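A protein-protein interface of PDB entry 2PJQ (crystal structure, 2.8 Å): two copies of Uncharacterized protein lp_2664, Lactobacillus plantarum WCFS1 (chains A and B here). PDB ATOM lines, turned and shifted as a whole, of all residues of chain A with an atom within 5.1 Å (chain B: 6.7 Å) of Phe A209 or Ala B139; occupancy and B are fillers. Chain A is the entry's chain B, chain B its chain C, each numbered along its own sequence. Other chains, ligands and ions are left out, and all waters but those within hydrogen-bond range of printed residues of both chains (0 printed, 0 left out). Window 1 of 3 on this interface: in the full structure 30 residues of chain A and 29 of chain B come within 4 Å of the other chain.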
ATOM      1  N   ILE A 138      -2.238   0.725  10.864  1.00  0.00           N
ATOM      2  CA  ILE A 138      -3.413   1.370  10.277  1.00  0.00           C
ATOM      3  C   ILE A 138      -2.986   2.140   9.022  1.00  0.00           C
ATOM      4  O   ILE A 138      -3.485   1.896   7.919  1.00  0.00           O
ATOM      5  CB  ILE A 138      -4.046   2.376  11.248  1.00  0.00           C
ATOM      6  CG1 ILE A 138      -4.584   1.642  12.485  1.00  0.00           C
ATOM      7  CG2 ILE A 138      -5.135   3.161  10.531  1.00  0.00           C
ATOM      8  CD1 ILE A 138      -5.056   2.564  13.596  1.00  0.00           C
ATOM      9  N   LEU A 142      -4.157   0.895   5.087  1.00  0.00           N
ATOM     10  CA  LEU A 142      -4.904   1.650   4.096  1.00  0.00           C
ATOM     11  C   LEU A 142      -4.047   2.293   3.009  1.00  0.00           C
ATOM     12  O   LEU A 142      -4.503   2.495   1.880  1.00  0.00           O
ATOM     13  CB  LEU A 142      -5.779   2.718   4.780  1.00  0.00           C
ATOM     14  CG  LEU A 142      -7.063   2.070   5.295  1.00  0.00           C
ATOM     15  CD1 LEU A 142      -6.843   1.489   6.698  1.00  0.00           C
ATOM     16  CD2 LEU A 142      -8.158   3.091   5.274  1.00  0.00           C
ATOM     17  N   ILE A 152     -12.323   0.124   0.529  1.00  0.00           N
ATOM     18  CA  ILE A 152     -12.127   0.360   1.953  1.00  0.00           C
ATOM     19  C   ILE A 152     -13.070  -0.408   2.858  1.00  0.00           C
ATOM     20  O   ILE A 152     -12.661  -0.888   3.911  1.00  0.00           O
ATOM     21  CB  ILE A 152     -12.256   1.862   2.318  1.00  0.00           C
ATOM     22  CG1 ILE A 152     -11.403   2.711   1.380  1.00  0.00           C
ATOM     23  CG2 ILE A 152     -11.774   2.093   3.753  1.00  0.00           C
ATOM     24  CD1 ILE A 152     -11.608   4.204   1.545  1.00  0.00           C
ATOM     25  N   ILE A 176     -11.029  -2.690   5.628  1.00  0.00           N
ATOM     26  CA  ILE A 176     -11.443  -2.950   6.995  1.00  0.00           C
ATOM     27  C   ILE A 176     -11.359  -4.442   7.295  1.00  0.00           C
ATOM     28  O   ILE A 176     -10.813  -4.837   8.322  1.00  0.00           O
ATOM     29  CB  ILE A 176     -12.892  -2.466   7.256  1.00  0.00           C
ATOM     30  CG1 ILE A 176     -12.973  -0.940   7.140  1.00  0.00           C
ATOM     31  CG2 ILE A 176     -13.342  -2.896   8.650  1.00  0.00           C
ATOM     32  CD1 ILE A 176     -12.296  -0.182   8.276  1.00  0.00           C
ATOM     33  N   PHE A 179      -8.289  -6.043   9.013  1.00  0.00           N
ATOM     34  CA  PHE A 179      -8.033  -6.023  10.448  1.00  0.00           C
ATOM     35  C   PHE A 179      -8.669  -7.279  11.021  1.00  0.00           C
ATOM     36  O   PHE A 179      -8.016  -8.054  11.706  1.00  0.00           O
ATOM     37  CB  PHE A 179      -8.628  -4.776  11.115  1.00  0.00           C
ATOM     38  CG  PHE A 179      -7.957  -3.500  10.715  1.00  0.00           C
ATOM     39  CD1 PHE A 179      -8.218  -2.919   9.486  1.00  0.00           C
ATOM     40  CD2 PHE A 179      -7.020  -2.910  11.535  1.00  0.00           C
ATOM     41  CE1 PHE A 179      -7.550  -1.760   9.080  1.00  0.00           C
ATOM     42  CE2 PHE A 179      -6.345  -1.752  11.133  1.00  0.00           C
ATOM     43  CZ  PHE A 179      -6.615  -1.183   9.904  1.00  0.00           C
ATOM     44  N   VAL A 205      -5.559   0.764  19.506  1.00  0.00           N
ATOM     45  CA  VAL A 205      -5.684   1.798  18.480  1.00  0.00           C
ATOM     46  C   VAL A 205      -6.363   1.288  17.224  1.00  0.00           C
ATOM     47  O   VAL A 205      -7.192   1.959  16.634  1.00  0.00           O
ATOM     48  CB  VAL A 205      -4.296   2.316  18.062  1.00  0.00           C
ATOM     49  CG1 VAL A 205      -4.437   3.696  17.439  1.00  0.00           C
ATOM     50  CG2 VAL A 205      -3.343   2.318  19.273  1.00  0.00           C
ATOM     51  N   MET A 206      -5.974   0.100  16.798  1.00  0.00           N
ATOM     52  CA  MET A 206      -6.553  -0.480  15.614  1.00  0.00           C
ATOM     53  C   MET A 206      -8.026  -0.697  15.885  1.00  0.00           C
ATOM     54  O   MET A 206      -8.858  -0.392  15.029  1.00  0.00           O
ATOM     55  CB  MET A 206      -5.872  -1.802  15.275  1.00  0.00           C
ATOM     56  CG  MET A 206      -4.389  -1.703  14.973  1.00  0.00           C
ATOM     57  SD  MET A 206      -3.674  -3.451  14.499  1.00  0.00           S
ATOM     58  CE  MET A 206      -3.663  -3.272  12.583  1.00  0.00           C
ATOM     59  N   HIS A 207      -8.353  -1.214  17.073  1.00  0.00           N
ATOM     60  CA  HIS A 207      -9.759  -1.443  17.429  1.00  0.00           C
ATOM     61  C   HIS A 207     -10.577  -0.157  17.501  1.00  0.00           C
ATOM     62  O   HIS A 207     -11.743  -0.155  17.131  1.00  0.00           O
ATOM     63  CB  HIS A 207      -9.896  -2.213  18.747  1.00  0.00           C
ATOM     64  CG  HIS A 207      -9.895  -3.695  18.573  1.00  0.00           C
ATOM     65  ND1 HIS A 207      -8.755  -4.458  18.711  1.00  0.00           N
ATOM     66  CD2 HIS A 207     -10.870  -4.545  18.180  1.00  0.00           C
ATOM     67  CE1 HIS A 207      -9.028  -5.714  18.404  1.00  0.00           C
ATOM     68  NE2 HIS A 207     -10.304  -5.795  18.075  1.00  0.00           N
ATOM     69  N   GLU A 208      -9.981   0.930  17.981  1.00  0.00           N
ATOM     70  CA  GLU A 208     -10.689   2.207  18.027  1.00  0.00           C
ATOM     71  C   GLU A 208     -10.947   2.707  16.600  1.00  0.00           C
ATOM     72  O   GLU A 208     -11.955   3.371  16.327  1.00  0.00           O
ATOM     73  CB  GLU A 208      -9.875   3.248  18.804  1.00  0.00           C
ATOM     74  CG  GLU A 208     -10.177   3.251  20.306  1.00  0.00           C
ATOM     75  CD  GLU A 208      -8.987   3.695  21.136  1.00  0.00           C
ATOM     76  OE1 GLU A 208      -8.525   4.841  20.934  1.00  0.00           O
ATOM     77  OE2 GLU A 208      -8.516   2.895  21.986  1.00  0.00           O
ATOM     78  N   PHE A 209     -10.037   2.364  15.693  1.00  0.00           N
ATOM     79  CA  PHE A 209     -10.152   2.772  14.305  1.00  0.00           C
ATOM     80  C   PHE A 209     -11.260   2.021  13.574  1.00  0.00           C
ATOM     81  O   PHE A 209     -12.122   2.650  12.967  1.00  0.00           O
ATOM     82  CB  PHE A 209      -8.816   2.583  13.578  1.00  0.00           C
ATOM     83  CG  PHE A 209      -8.871   2.922  12.121  1.00  0.00           C
ATOM     84  CD1 PHE A 209      -9.060   4.234  11.701  1.00  0.00           C
ATOM     85  CD2 PHE A 209      -8.781   1.922  11.161  1.00  0.00           C
ATOM     86  CE1 PHE A 209      -9.160   4.546  10.334  1.00  0.00           C
ATOM     87  CE2 PHE A 209      -8.883   2.223   9.793  1.00  0.00           C
ATOM     88  CZ  PHE A 209      -9.073   3.540   9.383  1.00  0.00           C
ATOM     89  N   VAL A 210     -11.244   0.689  13.620  1.00  0.00           N
ATOM     90  CA  VAL A 210     -12.275  -0.106  12.951  1.00  0.00           C
ATOM     91  C   VAL A 210     -13.656   0.174  13.567  1.00  0.00           C
ATOM     92  O   VAL A 210     -14.691   0.124  12.888  1.00  0.00           O
ATOM     93  CB  VAL A 210     -11.965  -1.612  13.055  1.00  0.00           C
ATOM     94  CG1 VAL A 210     -12.979  -2.435  12.257  1.00  0.00           C
ATOM     95  CG2 VAL A 210     -10.568  -1.867  12.553  1.00  0.00           C
ATOM     96  N   ASP A 211     -13.674   0.475  14.860  1.00  0.00           N
ATOM     97  CA  ASP A 211     -14.927   0.767  15.532  1.00  0.00           C
ATOM     98  C   ASP A 211     -15.422   2.159  15.150  1.00  0.00           C
ATOM     99  O   ASP A 211     -16.515   2.304  14.602  1.00  0.00           O
ATOM    100  CB  ASP A 211     -14.753   0.599  17.045  1.00  0.00           C
ATOM    101  CG  ASP A 211     -14.657  -0.875  17.450  1.00  0.00           C
ATOM    102  OD1 ASP A 211     -14.730  -1.744  16.548  1.00  0.00           O
ATOM    103  OD2 ASP A 211     -14.514  -1.176  18.653  1.00  0.00           O
ATOM    104  N   GLN A 212     -14.622   3.184  15.406  1.00  0.00           N
ATOM    105  CA  GLN A 212     -15.027   4.533  15.029  1.00  0.00           C
ATOM    106  C   GLN A 212     -15.346   4.649  13.535  1.00  0.00           C
ATOM    107  O   GLN A 212     -16.152   5.484  13.132  1.00  0.00           O
ATOM    108  CB  GLN A 212     -13.940   5.535  15.398  1.00  0.00           C
ATOM    109  CG  GLN A 212     -14.137   6.121  16.771  1.00  0.00           C
ATOM    110  CD  GLN A 212     -15.546   6.619  16.953  1.00  0.00           C
ATOM    111  OE1 GLN A 212     -16.387   5.936  17.544  1.00  0.00           O
ATOM    112  NE2 GLN A 212     -15.827   7.809  16.419  1.00  0.00           N
ATOM    113  N   PHE A 213     -14.716   3.815  12.715  1.00  0.00           N
ATOM    114  CA  PHE A 213     -14.958   3.844  11.279  1.00  0.00           C
ATOM    115  C   PHE A 213     -16.365   3.334  10.943  1.00  0.00           C
ATOM    116  O   PHE A 213     -17.029   3.872  10.058  1.00  0.00           O
ATOM    117  CB  PHE A 213     -13.897   3.007  10.540  1.00  0.00           C
ATOM    118  CG  PHE A 213     -14.086   2.963   9.042  1.00  0.00           C
ATOM    119  CD1 PHE A 213     -15.033   2.121   8.469  1.00  0.00           C
ATOM    120  CD2 PHE A 213     -13.324   3.777   8.207  1.00  0.00           C
ATOM    121  CE1 PHE A 213     -15.225   2.088   7.080  1.00  0.00           C
ATOM    122  CE2 PHE A 213     -13.503   3.756   6.820  1.00  0.00           C
ATOM    123  CZ  PHE A 213     -14.454   2.908   6.256  1.00  0.00           C
ATOM    124  N   LYS A 214     -16.823   2.307  11.653  1.00  0.00           N
ATOM    125  CA  LYS A 214     -18.143   1.745  11.391  1.00  0.00           C
ATOM    126  C   LYS A 214     -19.224   2.517  12.116  1.00  0.00           C
ATOM    127  O   LYS A 214     -20.394   2.458  11.745  1.00  0.00           O
ATOM    128  CB  LYS A 214     -18.176   0.271  11.783  1.00  0.00           C
ATOM    129  CG  LYS A 214     -17.036  -0.485  11.149  1.00  0.00           C
ATOM    130  CD  LYS A 214     -17.463  -1.805  10.568  1.00  0.00           C
ATOM    131  CE  LYS A 214     -17.577  -2.856  11.627  1.00  0.00           C
ATOM    132  NZ  LYS A 214     -17.837  -4.141  10.947  1.00  0.00           N
ATOM    133  N   GLY B 134     -12.357  12.170  11.203  1.00  0.00           N
ATOM    134  CA  GLY B 134     -12.884  11.000  11.882  1.00  0.00           C
ATOM    135  C   GLY B 134     -12.116   9.739  11.503  1.00  0.00           C
ATOM    136  O   GLY B 134     -10.989   9.799  11.000  1.00  0.00           O
ATOM    137  N   ALA B 135     -12.710   8.581  11.742  1.00  0.00           N
ATOM    138  CA  ALA B 135     -12.032   7.353  11.407  1.00  0.00           C
ATOM    139  C   ALA B 135     -12.059   7.257   9.895  1.00  0.00           C
ATOM    140  O   ALA B 135     -11.085   6.845   9.260  1.00  0.00           O
ATOM    141  CB  ALA B 135     -12.753   6.180  12.030  1.00  0.00           C
ATOM    142  N   ILE B 136     -13.184   7.649   9.310  1.00  0.00           N
ATOM    143  CA  ILE B 136     -13.316   7.593   7.866  1.00  0.00           C
ATOM    144  C   ILE B 136     -12.364   8.600   7.252  1.00  0.00           C
ATOM    145  O   ILE B 136     -11.812   8.362   6.164  1.00  0.00           O
ATOM    146  CB  ILE B 136     -14.753   7.894   7.422  1.00  0.00           C
ATOM    147  CG1 ILE B 136     -15.657   6.692   7.737  1.00  0.00           C
ATOM    148  CG2 ILE B 136     -14.775   8.219   5.933  1.00  0.00           C
ATOM    149  CD1 ILE B 136     -17.141   6.956   7.502  1.00  0.00           C
ATOM    150  N   GLY B 137     -12.167   9.714   7.962  1.00  0.00           N
ATOM    151  CA  GLY B 137     -11.261  10.744   7.494  1.00  0.00           C
ATOM    152  C   GLY B 137      -9.846  10.206   7.438  1.00  0.00           C
ATOM    153  O   GLY B 137      -9.108  10.461   6.488  1.00  0.00           O
ATOM    154  N   ILE B 138      -9.465   9.448   8.458  1.00  0.00           N
ATOM    155  CA  ILE B 138      -8.132   8.860   8.512  1.00  0.00           C
ATOM    156  C   ILE B 138      -7.950   7.951   7.304  1.00  0.00           C
ATOM    157  O   ILE B 138      -6.975   8.061   6.572  1.00  0.00           O
ATOM    158  CB  ILE B 138      -7.945   7.974   9.743  1.00  0.00           C
ATOM    159  CG1 ILE B 138      -8.228   8.750  11.027  1.00  0.00           C
ATOM    160  CG2 ILE B 138      -6.555   7.411   9.747  1.00  0.00           C
ATOM    161  CD1 ILE B 138      -8.228   7.868  12.266  1.00  0.00           C
ATOM    162  N   ALA B 139      -8.900   7.038   7.117  1.00  0.00           N
ATOM    163  CA  ALA B 139      -8.851   6.091   6.012  1.00  0.00           C
ATOM    164  C   ALA B 139      -8.665   6.797   4.660  1.00  0.00           C
ATOM    165  O   ALA B 139      -7.710   6.518   3.934  1.00  0.00           O
ATOM    166  CB  ALA B 139     -10.116   5.240   6.010  1.00  0.00           C
ATOM    167  N   ARG B 140      -9.575   7.719   4.338  1.00  0.00           N
ATOM    168  CA  ARG B 140      -9.504   8.453   3.077  1.00  0.00           C
ATOM    169  C   ARG B 140      -8.176   9.213   2.997  1.00  0.00           C
ATOM    170  O   ARG B 140      -7.514   9.228   1.962  1.00  0.00           O
ATOM    171  CB  ARG B 140     -10.710   9.390   2.951  1.00  0.00           C
ATOM    172  CG  ARG B 140     -12.044   8.618   2.823  1.00  0.00           C
ATOM    173  CD  ARG B 140     -13.287   9.459   2.429  1.00  0.00           C
ATOM    174  NE  ARG B 140     -13.037  10.304   1.271  1.00  0.00           N
ATOM    175  CZ  ARG B 140     -12.889  11.620   1.338  1.00  0.00           C
ATOM    176  NH1 ARG B 140     -12.986  12.234   2.505  1.00  0.00           N
ATOM    177  NH2 ARG B 140     -12.599  12.316   0.250  1.00  0.00           N
ATOM    178  N   ALA B 141      -7.769   9.810   4.107  1.00  0.00           N
ATOM    179  CA  ALA B 141      -6.512  10.538   4.157  1.00  0.00           C
ATOM    180  C   ALA B 141      -5.347   9.741   3.569  1.00  0.00           C
ATOM    181  O   ALA B 141      -4.721  10.172   2.610  1.00  0.00           O
ATOM    182  CB  ALA B 141      -6.199  10.889   5.584  1.00  0.00           C
ATOM    183  N   LEU B 142      -5.067   8.576   4.155  1.00  0.00           N
ATOM    184  CA  LEU B 142      -3.957   7.723   3.733  1.00  0.00           C
ATOM    185  C   LEU B 142      -4.197   6.886   2.501  1.00  0.00           C
ATOM    186  O   LEU B 142      -3.271   6.615   1.742  1.00  0.00           O
ATOM    187  CB  LEU B 142      -3.534   6.806   4.877  1.00  0.00           C
ATOM    188  CG  LEU B 142      -2.655   7.530   5.898  1.00  0.00           C
ATOM    189  CD1 LEU B 142      -3.347   7.528   7.239  1.00  0.00           C
ATOM    190  CD2 LEU B 142      -1.287   6.866   5.969  1.00  0.00           C
ATOM    191  N   TYR B 143      -5.430   6.445   2.316  1.00  0.00           N
ATOM    192  CA  TYR B 143      -5.747   5.670   1.140  1.00  0.00           C
ATOM    193  C   TYR B 143      -5.239   6.560  -0.005  1.00  0.00           C
ATOM    194  O   TYR B 143      -4.355   6.164  -0.795  1.00  0.00           O
ATOM    195  CB  TYR B 143      -7.257   5.456   1.076  1.00  0.00           C
ATOM    196  CG  TYR B 143      -7.751   4.649  -0.103  1.00  0.00           C
ATOM    197  CD1 TYR B 143      -7.879   5.221  -1.371  1.00  0.00           C
ATOM    198  CD2 TYR B 143      -8.145   3.323   0.063  1.00  0.00           C
ATOM    199  CE1 TYR B 143      -8.399   4.495  -2.434  1.00  0.00           C
ATOM    200  CE2 TYR B 143      -8.658   2.592  -0.989  1.00  0.00           C
ATOM    201  CZ  TYR B 143      -8.790   3.182  -2.229  1.00  0.00           C
ATOM    202  OH  TYR B 143      -9.364   2.464  -3.239  1.00  0.00           O
ATOM    203  N   TYR B 144      -5.770   7.781  -0.052  1.00  0.00           N
ATOM    204  CA  TYR B 144      -5.373   8.765  -1.055  1.00  0.00           C
ATOM    205  C   TYR B 144      -3.867   8.892  -1.189  1.00  0.00           C
ATOM    206  O   TYR B 144      -3.357   8.923  -2.302  1.00  0.00           O
ATOM    207  CB  TYR B 144      -5.888  10.158  -0.719  1.00  0.00           C
ATOM    208  CG  TYR B 144      -5.462  11.161  -1.762  1.00  0.00           C
ATOM    209  CD1 TYR B 144      -6.116  11.218  -2.992  1.00  0.00           C
ATOM    210  CD2 TYR B 144      -4.376  12.014  -1.549  1.00  0.00           C
ATOM    211  CE1 TYR B 144      -5.707  12.089  -3.981  1.00  0.00           C
ATOM    212  CE2 TYR B 144      -3.954  12.893  -2.542  1.00  0.00           C
ATOM    213  CZ  TYR B 144      -4.627  12.924  -3.755  1.00  0.00           C
ATOM    214  OH  TYR B 144      -4.243  13.785  -4.755  1.00  0.00           O
ATOM    215  N   SER B 145      -3.163   9.021  -0.064  1.00  0.00           N
ATOM    216  CA  SER B 145      -1.704   9.148  -0.089  1.00  0.00           C
ATOM    217  C   SER B 145      -1.086   7.917  -0.750  1.00  0.00           C
ATOM    218  O   SER B 145      -0.202   8.036  -1.606  1.00  0.00           O
ATOM    219  CB  SER B 145      -1.143   9.301   1.329  1.00  0.00           C
ATOM    220  OG  SER B 145      -1.518  10.540   1.916  1.00  0.00           O
ATOM    221  N   PHE B 179      -2.849  16.055   8.503  1.00  0.00           N
ATOM    222  CA  PHE B 179      -3.743  16.244   9.625  1.00  0.00           C
ATOM    223  C   PHE B 179      -3.476  17.613  10.232  1.00  0.00           C
ATOM    224  O   PHE B 179      -4.398  18.371  10.488  1.00  0.00           O
ATOM    225  CB  PHE B 179      -3.510  15.146  10.669  1.00  0.00           C
ATOM    226  CG  PHE B 179      -3.826  13.772  10.172  1.00  0.00           C
ATOM    227  CD1 PHE B 179      -3.015  13.158   9.242  1.00  0.00           C
ATOM    228  CD2 PHE B 179      -4.990  13.120  10.587  1.00  0.00           C
ATOM    229  CE1 PHE B 179      -3.352  11.924   8.726  1.00  0.00           C
ATOM    230  CE2 PHE B 179      -5.337  11.878  10.076  1.00  0.00           C
ATOM    231  CZ  PHE B 179      -4.521  11.277   9.141  1.00  0.00           C
ATOM    232  N   VAL B 205     -10.524  10.990  17.534  1.00  0.00           N
ATOM    233  CA  VAL B 205      -9.947   9.770  16.967  1.00  0.00           C
ATOM    234  C   VAL B 205      -8.708  10.063  16.131  1.00  0.00           C
ATOM    235  O   VAL B 205      -7.745   9.299  16.149  1.00  0.00           O
ATOM    236  CB  VAL B 205     -10.951   9.011  16.065  1.00  0.00           C
ATOM    237  CG1 VAL B 205     -10.415   7.610  15.760  1.00  0.00           C
ATOM    238  CG2 VAL B 205     -12.336   8.953  16.743  1.00  0.00           C
ATOM    239  N   MET B 206      -8.735  11.163  15.391  1.00  0.00           N
ATOM    240  CA  MET B 206      -7.596  11.519  14.562  1.00  0.00           C
ATOM    241  C   MET B 206      -6.375  11.730  15.422  1.00  0.00           C
ATOM    242  O   MET B 206      -5.263  11.395  15.018  1.00  0.00           O
ATOM    243  CB  MET B 206      -7.873  12.790  13.783  1.00  0.00           C
ATOM    244  CG  MET B 206      -9.229  12.788  13.148  1.00  0.00           C
ATOM    245  SD  MET B 206      -9.281  13.957  11.656  1.00  0.00           S
ATOM    246  CE  MET B 206      -9.237  12.583  10.302  1.00  0.00           C
ATOM    247  N   PHE B 209      -4.787   8.651  16.738  1.00  0.00           N
ATOM    248  CA  PHE B 209      -4.017   8.014  15.664  1.00  0.00           C
ATOM    249  C   PHE B 209      -2.692   8.695  15.369  1.00  0.00           C
ATOM    250  O   PHE B 209      -1.719   8.028  15.029  1.00  0.00           O
ATOM    251  CB  PHE B 209      -4.862   8.000  14.384  1.00  0.00           C
ATOM    252  CG  PHE B 209      -4.106   7.622  13.135  1.00  0.00           C
ATOM    253  CD1 PHE B 209      -3.913   6.287  12.793  1.00  0.00           C
ATOM    254  CD2 PHE B 209      -3.642   8.613  12.258  1.00  0.00           C
ATOM    255  CE1 PHE B 209      -3.280   5.938  11.590  1.00  0.00           C
ATOM    256  CE2 PHE B 209      -3.012   8.278  11.060  1.00  0.00           C
ATOM    257  CZ  PHE B 209      -2.829   6.934  10.724  1.00  0.00           C
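Of chain B, only Ala B135 (3.2 Å), Ile B138 (3.7 Å) and Ala B139 (3.9 Å) come within 4 Å of Phe A209. Ala B139 touches three residues of chain A. Of the printed residues of chain A, Val B205 touches Gln A212 (3.4 Å). Printed residues of chain B within 4 Å of Leu A142: Ala B139 (3.0 Å) and Tyr B143 (3.5 Å). Printed residues of chain B within 4 Å of Ile A138: Phe B209 (3.5 Å). Of the printed residues of chain A, Ile B136 touches Phe A213 (3.8 Å). Lys A214 touches none of the printed residues of chain B. The nearest residue of chain B that does not touch Phe A209 is Val B205 (5.1 Å).
Leu A142 touches Ala B139 (CD2 to CB, 3.0 Å). CA of Tyr B143 touches O of Leu A142, 3.5 Å away. Ile A152 touches Tyr B143. O of Ala B135 touches CE1 of Phe A209, at 3.2 Å. Ile B138 touches Phe A209. Ala B135 touches Gln A212 (CB to C, 3.4 Å). CG2 of Val B205 touches CG of Gln A212 (3.4 Å). CB of Ala B135 touches N of Phe A213, at 3.1 Å. CE2 of Phe A213 touches CG1 of Ile B136 (3.8 Å). Phe A213 touches Ala B139.
Hydrophobic or aromatic side chains of chain A that line the printed part of chain B: Ile A138, Leu A142, Ile A152, Phe A209 and Phe A213. Along chain A the printed residues that touch a printed residue of chain B span positions 138 to 213. Among the printed residues, 12 pairs touch across the chains.
Ile A138 touches Phe B209, and with the chains exchanged Phe A209 touches Ile B138. 6 positions are printed for both chains.
O of Ile A152 lies within hydrogen-bond range of N of Ile A176 (3.0 Å).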
